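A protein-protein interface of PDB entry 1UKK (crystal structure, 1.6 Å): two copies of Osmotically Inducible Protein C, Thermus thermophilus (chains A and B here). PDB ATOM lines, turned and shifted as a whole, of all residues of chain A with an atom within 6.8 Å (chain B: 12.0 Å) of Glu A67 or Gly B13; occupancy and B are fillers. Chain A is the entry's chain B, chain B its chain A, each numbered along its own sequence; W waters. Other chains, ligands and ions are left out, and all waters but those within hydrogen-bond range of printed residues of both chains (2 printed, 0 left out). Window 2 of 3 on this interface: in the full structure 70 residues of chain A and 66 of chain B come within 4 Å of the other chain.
O of Pro A73 lies within hydrogen-bond range of N of Gly B12 (3.1 Å). The backbone NH of Leu B14 is in hydrogen-bond range of the side-chain carboxylate of Glu A67 (2.9 Å). The guanidinium group (NH1) of Arg B37 is in hydrogen-bond range of the side-chain sulfur (SD) of Met A60, 3.6 Å away.
NE1 of Trp B10 is in hydrogen-bond range of O of Gly B12, 2.9 Å away. NE1 of Trp B10 is in hydrogen-bond range of O of Gly B13 (3.1 Å). NH2 of Arg B15 is in hydrogen-bond range of OH of Tyr B34 (3.2 Å). N of Ser B33 sits at hydrogen-bond distance from OG of Ser B36 (2.9 Å).
Met A60 touches Trp B10 (CE to CH2, 3.7 Å). Leu B14 touches Met A60. Met A60 touches Ser B33. Met A60 touches Tyr B34. Met A60 touches Phe B38. Ala A63 touches Trp B10. Ala A63 touches Gly B12 (CB to O, 3.5 Å). Ala A64 touches Leu B14. Gly B13 touches Glu A67 (CA to OE2, 3.5 Å).
Gly B13 touches just one residue of chain A: Glu A67 (3.5 Å). Of chain B, only Leu B14 comes within 4 Å of Ala A64. No residue of chain B comes within 4 Å of Glu A69. No residue of chain B comes within 4 Å of Pro A72. Of the printed residues of chain A, Tyr B34 touches Met A60 (3.7 Å). Of the printed residues of chain A, Leu B14 touches Met A60 (3.5 Å), Ala A64 (3.98 Å) and Glu A67 (2.9 Å). Of the printed residues of chain B, Met A60 touches Trp B10 (3.7 Å), Leu B14 (3.5 Å), Ser B33 (3.98 Å), Tyr B34 (3.7 Å), Arg B37 (3.6 Å) and Phe B38 (3.6 Å). Printed residues of chain A within 4 Å of Gly B12: Ala A63 and Pro A73. Of the printed residues of chain A, Phe B38 touches Met A60. The nearest printed residue of chain B that does not touch Met A60 is Tyr B32 (4.1 Å).
Of the 19 printed residues of chain B, 8 touch a printed residue of chain A. Hydrophobic or aromatic side chains of chain B within 4 Å of the printed part of chain A: Trp B10, Leu B14 and Phe B38. Of the 14 printed residues of chain A, 5 touch a printed residue of chain B.
No position is printed for both chains.
Water W2 lies within hydrogen-bond range of OE1 of Glu A67 (2.7 Å) and N of Arg B15 (2.9 Å). Water W1 lies within hydrogen-bond range of the backbone NH of Gln B16 (2.9 Å), the side-chain carboxylate of Glu A67 (3.1 Å) and the backbone NH of Arg B15 (3.4 Å).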
ATOM      1  N   MET A  60       0.325 -23.436  14.078  1.00  0.00           N
ATOM      2  CA  MET A  60       0.205 -22.337  15.042  1.00  0.00           C
ATOM      3  C   MET A  60       0.120 -22.817  16.499  1.00  0.00           C
ATOM      4  O   MET A  60       0.737 -22.236  17.420  1.00  0.00           O
ATOM      5  CB  MET A  60      -0.968 -21.453  14.657  1.00  0.00           C
ATOM      6  CG  MET A  60      -1.036 -20.164  15.397  1.00  0.00           C
ATOM      7  SD  MET A  60      -2.838 -19.413  15.025  1.00  0.00           S
ATOM      8  CE  MET A  60      -2.544 -17.654  15.728  1.00  0.00           C
ATOM      9  N   LEU A  62       1.201 -25.703  17.791  1.00  0.00           N
ATOM     10  CA  LEU A  62       2.516 -26.272  18.161  1.00  0.00           C
ATOM     11  C   LEU A  62       3.489 -25.130  18.481  1.00  0.00           C
ATOM     12  O   LEU A  62       4.178 -25.170  19.485  1.00  0.00           O
ATOM     13  CB  LEU A  62       3.046 -27.253  17.109  1.00  0.00           C
ATOM     14  CG  LEU A  62       4.452 -27.817  17.438  1.00  0.00           C
ATOM     15  CD1 LEU A  62       4.539 -28.443  18.761  1.00  0.00           C
ATOM     16  CD2 LEU A  62       4.787 -28.766  16.347  1.00  0.00           C
ATOM     17  N   ALA A  63       3.516 -24.113  17.634  1.00  0.00           N
ATOM     18  CA  ALA A  63       4.369 -22.935  17.896  1.00  0.00           C
ATOM     19  C   ALA A  63       4.008 -22.289  19.245  1.00  0.00           C
ATOM     20  O   ALA A  63       4.879 -21.963  20.072  1.00  0.00           O
ATOM     21  CB  ALA A  63       4.245 -21.952  16.784  1.00  0.00           C
ATOM     22  N   ALA A  64       2.724 -22.132  19.506  1.00  0.00           N
ATOM     23  CA  ALA A  64       2.289 -21.578  20.811  1.00  0.00           C
ATOM     24  C   ALA A  64       2.775 -22.403  22.026  1.00  0.00           C
ATOM     25  O   ALA A  64       3.303 -21.866  23.018  1.00  0.00           O
ATOM     26  CB  ALA A  64       0.810 -21.443  20.826  1.00  0.00           C
ATOM     27  N   SER A  65       2.595 -23.714  21.977  1.00  0.00           N
ATOM     28  CA  SER A  65       3.052 -24.593  23.039  1.00  0.00           C
ATOM     29  C   SER A  65       4.567 -24.542  23.244  1.00  0.00           C
ATOM     30  O   SER A  65       5.069 -24.385  24.347  1.00  0.00           O
ATOM     31  CB  SER A  65       2.650 -25.992  22.689  1.00  0.00           C
ATOM     32  OG  SER A  65       2.520 -26.751  23.873  1.00  0.00           O
ATOM     33  N   LEU A  66       5.281 -24.646  22.151  1.00  0.00           N
ATOM     34  CA  LEU A  66       6.773 -24.542  22.213  1.00  0.00           C
ATOM     35  C   LEU A  66       7.176 -23.227  22.873  1.00  0.00           C
ATOM     36  O   LEU A  66       8.028 -23.210  23.749  1.00  0.00           O
ATOM     37  CB  LEU A  66       7.322 -24.635  20.824  1.00  0.00           C
ATOM     38  CG  LEU A  66       7.231 -26.050  20.248  1.00  0.00           C
ATOM     39  CD1 LEU A  66       7.533 -26.002  18.793  1.00  0.00           C
ATOM     40  CD2 LEU A  66       8.144 -27.087  20.861  1.00  0.00           C
ATOM     41  N   GLU A  67       6.522 -22.143  22.480  1.00  0.00           N
ATOM     42  CA  GLU A  67       6.848 -20.849  23.082  1.00  0.00           C
ATOM     43  C   GLU A  67       6.582 -20.832  24.570  1.00  0.00           C
ATOM     44  O   GLU A  67       7.330 -20.212  25.342  1.00  0.00           O
ATOM     45  CB  GLU A  67       5.972 -19.776  22.427  1.00  0.00           C
ATOM     46  CG  GLU A  67       6.178 -18.356  22.982  1.00  0.00           C
ATOM     47  CD  GLU A  67       5.478 -17.273  22.188  1.00  0.00           C
ATOM     48  OE1 GLU A  67       4.224 -17.443  21.977  1.00  0.00           O
ATOM     49  OE2 GLU A  67       6.080 -16.258  21.795  1.00  0.00           O
ATOM     50  N   ARG A  68       5.486 -21.438  25.025  1.00  0.00           N
ATOM     51  CA  ARG A  68       5.161 -21.569  26.473  1.00  0.00           C
ATOM     52  C   ARG A  68       6.185 -22.327  27.278  1.00  0.00           C
ATOM     53  O   ARG A  68       6.264 -22.153  28.485  1.00  0.00           O
ATOM     54  CB  ARG A  68       3.767 -22.186  26.716  1.00  0.00           C
ATOM     55  CG  ARG A  68       2.562 -21.314  26.294  1.00  0.00           C
ATOM     56  CD  ARG A  68       1.210 -21.919  26.660  1.00  0.00           C
ATOM     57  NE  ARG A  68       0.959 -21.885  28.087  1.00  0.00           N
ATOM     58  CZ  ARG A  68       0.246 -20.949  28.693  1.00  0.00           C
ATOM     59  NH1 ARG A  68      -0.287 -19.957  27.999  1.00  0.00           N
ATOM     60  NH2 ARG A  68       0.055 -21.015  30.002  1.00  0.00           N
ATOM     61  N   GLU A  69       6.965 -23.167  26.609  1.00  0.00           N
ATOM     62  CA  GLU A  69       8.054 -23.923  27.217  1.00  0.00           C
ATOM     63  C   GLU A  69       9.405 -23.169  27.109  1.00  0.00           C
ATOM     64  O   GLU A  69      10.428 -23.633  27.601  1.00  0.00           O
ATOM     65  CB  GLU A  69       8.116 -25.325  26.606  1.00  0.00           C
ATOM     66  CG  GLU A  69       6.947 -26.214  27.039  1.00  0.00           C
ATOM     67  CD  GLU A  69       6.986 -26.546  28.497  1.00  0.00           C
ATOM     68  OE1 GLU A  69       8.077 -26.922  28.966  1.00  0.00           O
ATOM     69  OE2 GLU A  69       5.946 -26.382  29.182  1.00  0.00           O
ATOM     70  N   GLY A  70       9.366 -21.983  26.548  1.00  0.00           N
ATOM     71  CA  GLY A  70      10.525 -21.129  26.340  1.00  0.00           C
ATOM     72  C   GLY A  70      11.349 -21.420  25.114  1.00  0.00           C
ATOM     73  O   GLY A  70      12.469 -20.896  24.922  1.00  0.00           O
ATOM     74  N   PHE A  71      10.716 -22.141  24.188  1.00  0.00           N
ATOM     75  CA  PHE A  71      11.307 -22.516  22.904  1.00  0.00           C
ATOM     76  C   PHE A  71      10.444 -22.118  21.682  1.00  0.00           C
ATOM     77  O   PHE A  71      10.039 -22.997  20.892  1.00  0.00           O
ATOM     78  CB  PHE A  71      11.562 -24.024  22.841  1.00  0.00           C
ATOM     79  CG  PHE A  71      12.431 -24.610  23.988  1.00  0.00           C
ATOM     80  CD1 PHE A  71      13.786 -24.536  23.950  1.00  0.00           C
ATOM     81  CD2 PHE A  71      11.808 -25.208  25.066  1.00  0.00           C
ATOM     82  CE1 PHE A  71      14.539 -25.114  25.018  1.00  0.00           C
ATOM     83  CE2 PHE A  71      12.566 -25.762  26.119  1.00  0.00           C
ATOM     84  CZ  PHE A  71      13.933 -25.701  26.030  1.00  0.00           C
ATOM     85  N   PRO A  72      10.197 -20.825  21.475  1.00  0.00           N
ATOM     86  CA  PRO A  72       9.501 -20.351  20.240  1.00  0.00           C
ATOM     87  C   PRO A  72      10.227 -20.873  18.995  1.00  0.00           C
ATOM     88  O   PRO A  72      11.489 -20.786  18.859  1.00  0.00           O
ATOM     89  CB  PRO A  72       9.475 -18.846  20.400  1.00  0.00           C
ATOM     90  CG  PRO A  72      10.646 -18.556  21.352  1.00  0.00           C
ATOM     91  CD  PRO A  72      10.725 -19.710  22.291  1.00  0.00           C
ATOM     92  N   PRO A  73       9.477 -21.420  18.056  1.00  0.00           N
ATOM     93  CA  PRO A  73      10.121 -22.004  16.885  1.00  0.00           C
ATOM     94  C   PRO A  73      10.546 -20.990  15.866  1.00  0.00           C
ATOM     95  O   PRO A  73       9.906 -19.949  15.659  1.00  0.00           O
ATOM     96  CB  PRO A  73       9.053 -22.889  16.326  1.00  0.00           C
ATOM     97  CG  PRO A  73       7.831 -22.163  16.650  1.00  0.00           C
ATOM     98  CD  PRO A  73       8.014 -21.610  18.042  1.00  0.00           C
ATOM     99  N   ILE A 115       5.918 -32.285  23.515  1.00  0.00           N
ATOM    100  CA  ILE A 115       5.082 -31.082  23.258  1.00  0.00           C
ATOM    101  C   ILE A 115       4.190 -31.240  22.064  1.00  0.00           C
ATOM    102  O   ILE A 115       3.010 -30.880  22.151  1.00  0.00           O
ATOM    103  CB  ILE A 115       5.955 -29.794  23.179  1.00  0.00           C
ATOM    104  CG1 ILE A 115       6.569 -29.441  24.520  1.00  0.00           C
ATOM    105  CG2 ILE A 115       5.172 -28.615  22.737  1.00  0.00           C
ATOM    106  CD1 ILE A 115       7.726 -28.464  24.407  1.00  0.00           C
ATOM    107  N   VAL B   9       2.716 -23.401   7.071  1.00  0.00           N
ATOM    108  CA  VAL B   9       3.965 -23.076   7.764  1.00  0.00           C
ATOM    109  C   VAL B   9       3.720 -21.923   8.703  1.00  0.00           C
ATOM    110  O   VAL B   9       3.042 -20.970   8.362  1.00  0.00           O
ATOM    111  CB  VAL B   9       5.117 -22.651   6.810  1.00  0.00           C
ATOM    112  CG1 VAL B   9       6.492 -22.551   7.525  1.00  0.00           C
ATOM    113  CG2 VAL B   9       5.022 -23.241   5.338  1.00  0.00           C
ATOM    114  N   TRP B  10       4.272 -22.002   9.908  1.00  0.00           N
ATOM    115  CA  TRP B  10       4.130 -20.939  10.916  1.00  0.00           C
ATOM    116  C   TRP B  10       5.551 -20.594  11.358  1.00  0.00           C
ATOM    117  O   TRP B  10       6.356 -21.498  11.595  1.00  0.00           O
ATOM    118  CB  TRP B  10       3.291 -21.392  12.109  1.00  0.00           C
ATOM    119  CG  TRP B  10       3.141 -20.271  13.138  1.00  0.00           C
ATOM    120  CD1 TRP B  10       4.000 -19.992  14.133  1.00  0.00           C
ATOM    121  CD2 TRP B  10       2.144 -19.239  13.137  1.00  0.00           C
ATOM    122  NE1 TRP B  10       3.580 -18.877  14.830  1.00  0.00           N
ATOM    123  CE2 TRP B  10       2.439 -18.384  14.235  1.00  0.00           C
ATOM    124  CE3 TRP B  10       0.978 -19.011  12.393  1.00  0.00           C
ATOM    125  CZ2 TRP B  10       1.649 -17.291  14.550  1.00  0.00           C
ATOM    126  CZ3 TRP B  10       0.198 -17.959  12.708  1.00  0.00           C
ATOM    127  CH2 TRP B  10       0.529 -17.100  13.783  1.00  0.00           C
ATOM    128  N   GLU B  11       5.879 -19.318  11.485  1.00  0.00           N
ATOM    129  CA  GLU B  11       7.191 -18.892  11.931  1.00  0.00           C
ATOM    130  C   GLU B  11       7.028 -17.984  13.151  1.00  0.00           C
ATOM    131  O   GLU B  11       6.170 -17.094  13.180  1.00  0.00           O
ATOM    132  CB  GLU B  11       7.917 -18.173  10.852  1.00  0.00           C
ATOM    133  CG  GLU B  11       8.224 -19.106   9.683  1.00  0.00           C
ATOM    134  CD  GLU B  11       8.764 -18.390   8.451  1.00  0.00           C
ATOM    135  OE1 GLU B  11       8.250 -17.303   8.065  1.00  0.00           O
ATOM    136  OE2 GLU B  11       9.709 -18.958   7.858  1.00  0.00           O
ATOM    137  N   GLY B  12       7.813 -18.238  14.165  1.00  0.00           N
ATOM    138  CA  GLY B  12       7.767 -17.527  15.419  1.00  0.00           C
ATOM    139  C   GLY B  12       6.773 -17.993  16.438  1.00  0.00           C
ATOM    140  O   GLY B  12       6.123 -19.043  16.284  1.00  0.00           O
ATOM    141  N   GLY B  13       6.660 -17.226  17.524  1.00  0.00           N
ATOM    142  CA  GLY B  13       5.688 -17.525  18.545  1.00  0.00           C
ATOM    143  C   GLY B  13       4.254 -17.166  18.202  1.00  0.00           C
ATOM    144  O   GLY B  13       3.963 -16.824  17.057  1.00  0.00           O
ATOM    145  N   LEU B  14       3.389 -17.269  19.161  1.00  0.00           N
ATOM    146  CA  LEU B  14       1.959 -17.076  18.967  1.00  0.00           C
ATOM    147  C   LEU B  14       1.525 -15.690  18.548  1.00  0.00           C
ATOM    148  O   LEU B  14       0.868 -15.548  17.529  1.00  0.00           O
ATOM    149  CB  LEU B  14       1.135 -17.540  20.135  1.00  0.00           C
ATOM    150  CG  LEU B  14      -0.403 -17.305  20.065  1.00  0.00           C
ATOM    151  CD1 LEU B  14      -0.902 -18.081  18.831  1.00  0.00           C
ATOM    152  CD2 LEU B  14      -1.063 -17.692  21.338  1.00  0.00           C
ATOM    153  N   ARG B  15       1.799 -14.703  19.389  1.00  0.00           N
ATOM    154  CA  ARG B  15       1.289 -13.358  19.112  1.00  0.00           C
ATOM    155  C   ARG B  15       2.023 -12.544  18.106  1.00  0.00           C
ATOM    156  O   ARG B  15       1.389 -11.694  17.435  1.00  0.00           O
ATOM    157  CB  ARG B  15       1.016 -12.616  20.420  1.00  0.00           C
ATOM    158  CG  ARG B  15      -0.012 -13.257  21.289  1.00  0.00           C
ATOM    159  CD  ARG B  15      -0.263 -12.527  22.653  1.00  0.00           C
ATOM    160  NE  ARG B  15      -1.647 -12.810  23.058  1.00  0.00           N
ATOM    161  CZ  ARG B  15      -2.032 -13.928  23.670  1.00  0.00           C
ATOM    162  NH1 ARG B  15      -1.156 -14.874  24.052  1.00  0.00           N
ATOM    163  NH2 ARG B  15      -3.303 -14.121  23.913  1.00  0.00           N
ATOM    164  N   GLN B  16       3.330 -12.796  17.930  1.00  0.00           N
ATOM    165  CA  GLN B  16       4.163 -12.124  16.997  1.00  0.00           C
ATOM    166  C   GLN B  16       4.520 -12.891  15.749  1.00  0.00           C
ATOM    167  O   GLN B  16       5.067 -12.324  14.829  1.00  0.00           O
ATOM    168  CB  GLN B  16       5.433 -11.647  17.696  1.00  0.00           C
ATOM    169  CG  GLN B  16       5.182 -10.699  18.875  1.00  0.00           C
ATOM    170  CD  GLN B  16       4.377  -9.468  18.514  1.00  0.00           C
ATOM    171  OE1 GLN B  16       4.570  -8.882  17.453  1.00  0.00           O
ATOM    172  NE2 GLN B  16       3.427  -9.083  19.384  1.00  0.00           N
ATOM    173  N   GLY B  17       4.201 -14.177  15.727  1.00  0.00           N
ATOM    174  CA  GLY B  17       4.475 -14.968  14.531  1.00  0.00           C
ATOM    175  C   GLY B  17       3.478 -14.750  13.379  1.00  0.00           C
ATOM    176  O   GLY B  17       2.525 -13.969  13.457  1.00  0.00           O
ATOM    177  N   LYS B  18       3.743 -15.459  12.288  1.00  0.00           N
ATOM    178  CA  LYS B  18       2.818 -15.501  11.187  1.00  0.00           C
ATOM    179  C   LYS B  18       2.989 -16.789  10.412  1.00  0.00           C
ATOM    180  O   LYS B  18       4.017 -17.466  10.471  1.00  0.00           O
ATOM    181  CB  LYS B  18       3.055 -14.340  10.213  1.00  0.00           C
ATOM    182  CG  LYS B  18       4.389 -14.302   9.556  1.00  0.00           C
ATOM    183  CD  LYS B  18       4.896 -12.860   9.188  1.00  0.00           C
ATOM    184  CE  LYS B  18       3.910 -12.085   8.352  1.00  0.00           C
ATOM    185  NZ  LYS B  18       4.576 -10.973   7.554  1.00  0.00           N
ATOM    186  N   GLY B  19       1.953 -17.090   9.685  1.00  0.00           N
ATOM    187  CA  GLY B  19       1.932 -18.307   8.908  1.00  0.00           C
ATOM    188  C   GLY B  19       1.286 -18.184   7.532  1.00  0.00           C
ATOM    189  O   GLY B  19       0.724 -17.183   7.126  1.00  0.00           O
ATOM    190  N   VAL B  20       1.354 -19.280   6.775  1.00  0.00           N
ATOM    191  CA  VAL B  20       0.697 -19.349   5.467  1.00  0.00           C
ATOM    192  C   VAL B  20       0.138 -20.745   5.288  1.00  0.00           C
ATOM    193  O   VAL B  20       0.836 -21.744   5.556  1.00  0.00           O
ATOM    194  CB  VAL B  20       1.673 -19.096   4.319  1.00  0.00           C
ATOM    195  CG1 VAL B  20       0.967 -19.247   2.986  1.00  0.00           C
ATOM    196  CG2 VAL B  20       2.311 -17.623   4.383  1.00  0.00           C
ATOM    197  N   TYR B  32      -1.935 -15.955   7.516  1.00  0.00           N
ATOM    198  CA  TYR B  32      -2.723 -15.857   8.714  1.00  0.00           C
ATOM    199  C   TYR B  32      -1.830 -15.531   9.908  1.00  0.00           C
ATOM    200  O   TYR B  32      -0.608 -15.716   9.853  1.00  0.00           O
ATOM    201  CB  TYR B  32      -3.570 -17.151   8.892  1.00  0.00           C
ATOM    202  CG  TYR B  32      -2.770 -18.379   9.354  1.00  0.00           C
ATOM    203  CD1 TYR B  32      -1.927 -18.993   8.463  1.00  0.00           C
ATOM    204  CD2 TYR B  32      -2.907 -18.940  10.594  1.00  0.00           C
ATOM    205  CE1 TYR B  32      -1.196 -20.147   8.825  1.00  0.00           C
ATOM    206  CE2 TYR B  32      -2.217 -20.153  10.979  1.00  0.00           C
ATOM    207  CZ  TYR B  32      -1.326 -20.713  10.090  1.00  0.00           C
ATOM    208  OH  TYR B  32      -0.586 -21.835  10.423  1.00  0.00           O
ATOM    209  N   SER B  33      -2.421 -14.949  10.934  1.00  0.00           N
ATOM    210  CA  SER B  33      -1.658 -14.446  12.080  1.00  0.00           C
ATOM    211  C   SER B  33      -2.580 -14.493  13.317  1.00  0.00           C
ATOM    212  O   SER B  33      -3.760 -14.778  13.245  1.00  0.00           O
ATOM    213  CB  SER B  33      -1.161 -13.039  11.748  1.00  0.00           C
ATOM    214  OG  SER B  33      -2.264 -12.208  11.477  1.00  0.00           O
ATOM    215  N   TYR B  34      -2.071 -14.103  14.480  1.00  0.00           N
ATOM    216  CA  TYR B  34      -2.916 -13.953  15.642  1.00  0.00           C
ATOM    217  C   TYR B  34      -3.977 -12.860  15.384  1.00  0.00           C
ATOM    218  O   TYR B  34      -5.159 -13.153  15.642  1.00  0.00           O
ATOM    219  CB  TYR B  34      -2.025 -13.659  16.854  1.00  0.00           C
ATOM    220  CG  TYR B  34      -2.839 -13.688  18.117  1.00  0.00           C
ATOM    221  CD1 TYR B  34      -3.557 -12.572  18.476  1.00  0.00           C
ATOM    222  CD2 TYR B  34      -2.955 -14.823  18.910  1.00  0.00           C
ATOM    223  CE1 TYR B  34      -4.344 -12.594  19.610  1.00  0.00           C
ATOM    224  CE2 TYR B  34      -3.726 -14.843  20.047  1.00  0.00           C
ATOM    225  CZ  TYR B  34      -4.457 -13.680  20.360  1.00  0.00           C
ATOM    226  OH  TYR B  34      -5.299 -13.571  21.521  1.00  0.00           O
ATOM    227  N   PRO B  35      -3.577 -11.663  14.899  1.00  0.00           N
ATOM    228  CA  PRO B  35      -4.586 -10.646  14.550  1.00  0.00           C
ATOM    229  C   PRO B  35      -5.619 -11.110  13.520  1.00  0.00           C
ATOM    230  O   PRO B  35      -6.789 -10.829  13.716  1.00  0.00           O
ATOM    231  CB  PRO B  35      -3.761  -9.434  14.050  1.00  0.00           C
ATOM    232  CG  PRO B  35      -2.384  -9.648  14.495  1.00  0.00           C
ATOM    233  CD  PRO B  35      -2.213 -11.134  14.676  1.00  0.00           C
ATOM    234  N   SER B  36      -5.227 -11.828  12.470  1.00  0.00           N
ATOM    235  CA  SER B  36      -6.231 -12.256  11.430  1.00  0.00           C
ATOM    236  C   SER B  36      -7.122 -13.390  11.971  1.00  0.00           C
ATOM    237  O   SER B  36      -8.255 -13.552  11.481  1.00  0.00           O
ATOM    238  CB  SER B  36      -5.579 -12.645  10.111  1.00  0.00           C
ATOM    239  OG  SER B  36      -5.042 -13.964  10.178  1.00  0.00           O
ATOM    240  N   ARG B  37      -6.680 -14.187  12.955  1.00  0.00           N
ATOM    241  CA  ARG B  37      -7.494 -15.258  13.453  1.00  0.00           C
ATOM    242  C   ARG B  37      -8.383 -14.910  14.624  1.00  0.00           C
ATOM    243  O   ARG B  37      -9.533 -15.276  14.683  1.00  0.00           O
ATOM    244  CB  ARG B  37      -6.589 -16.453  13.797  1.00  0.00           C
ATOM    245  CG  ARG B  37      -7.334 -17.601  14.214  1.00  0.00           C
ATOM    246  CD  ARG B  37      -6.535 -18.918  14.293  1.00  0.00           C
ATOM    247  NE  ARG B  37      -7.444 -20.074  14.404  1.00  0.00           N
ATOM    248  CZ  ARG B  37      -7.047 -21.285  14.747  1.00  0.00           C
ATOM    249  NH1 ARG B  37      -5.791 -21.511  15.081  1.00  0.00           N
ATOM    250  NH2 ARG B  37      -7.909 -22.312  14.768  1.00  0.00           N
ATOM    251  N   PHE B  38      -7.827 -14.172  15.586  1.00  0.00           N
ATOM    252  CA  PHE B  38      -8.544 -13.843  16.792  1.00  0.00           C
ATOM    253  C   PHE B  38      -9.097 -12.410  16.830  1.00  0.00           C
ATOM    254  O   PHE B  38     -10.022 -12.157  17.623  1.00  0.00           O
ATOM    255  CB  PHE B  38      -7.585 -14.097  17.933  1.00  0.00           C
ATOM    256  CG  PHE B  38      -7.196 -15.554  18.039  1.00  0.00           C
ATOM    257  CD1 PHE B  38      -8.124 -16.496  18.467  1.00  0.00           C
ATOM    258  CD2 PHE B  38      -5.965 -15.972  17.637  1.00  0.00           C
ATOM    259  CE1 PHE B  38      -7.776 -17.840  18.501  1.00  0.00           C
ATOM    260  CE2 PHE B  38      -5.588 -17.312  17.701  1.00  0.00           C
ATOM    261  CZ  PHE B  38      -6.486 -18.238  18.129  1.00  0.00           C
HETATM  262  O   HOH W   1       5.162 -14.207  19.694  1.00  0.00           O
HETATM  263  O   HOH W   2       2.975 -15.083  21.970  1.00  0.00           O
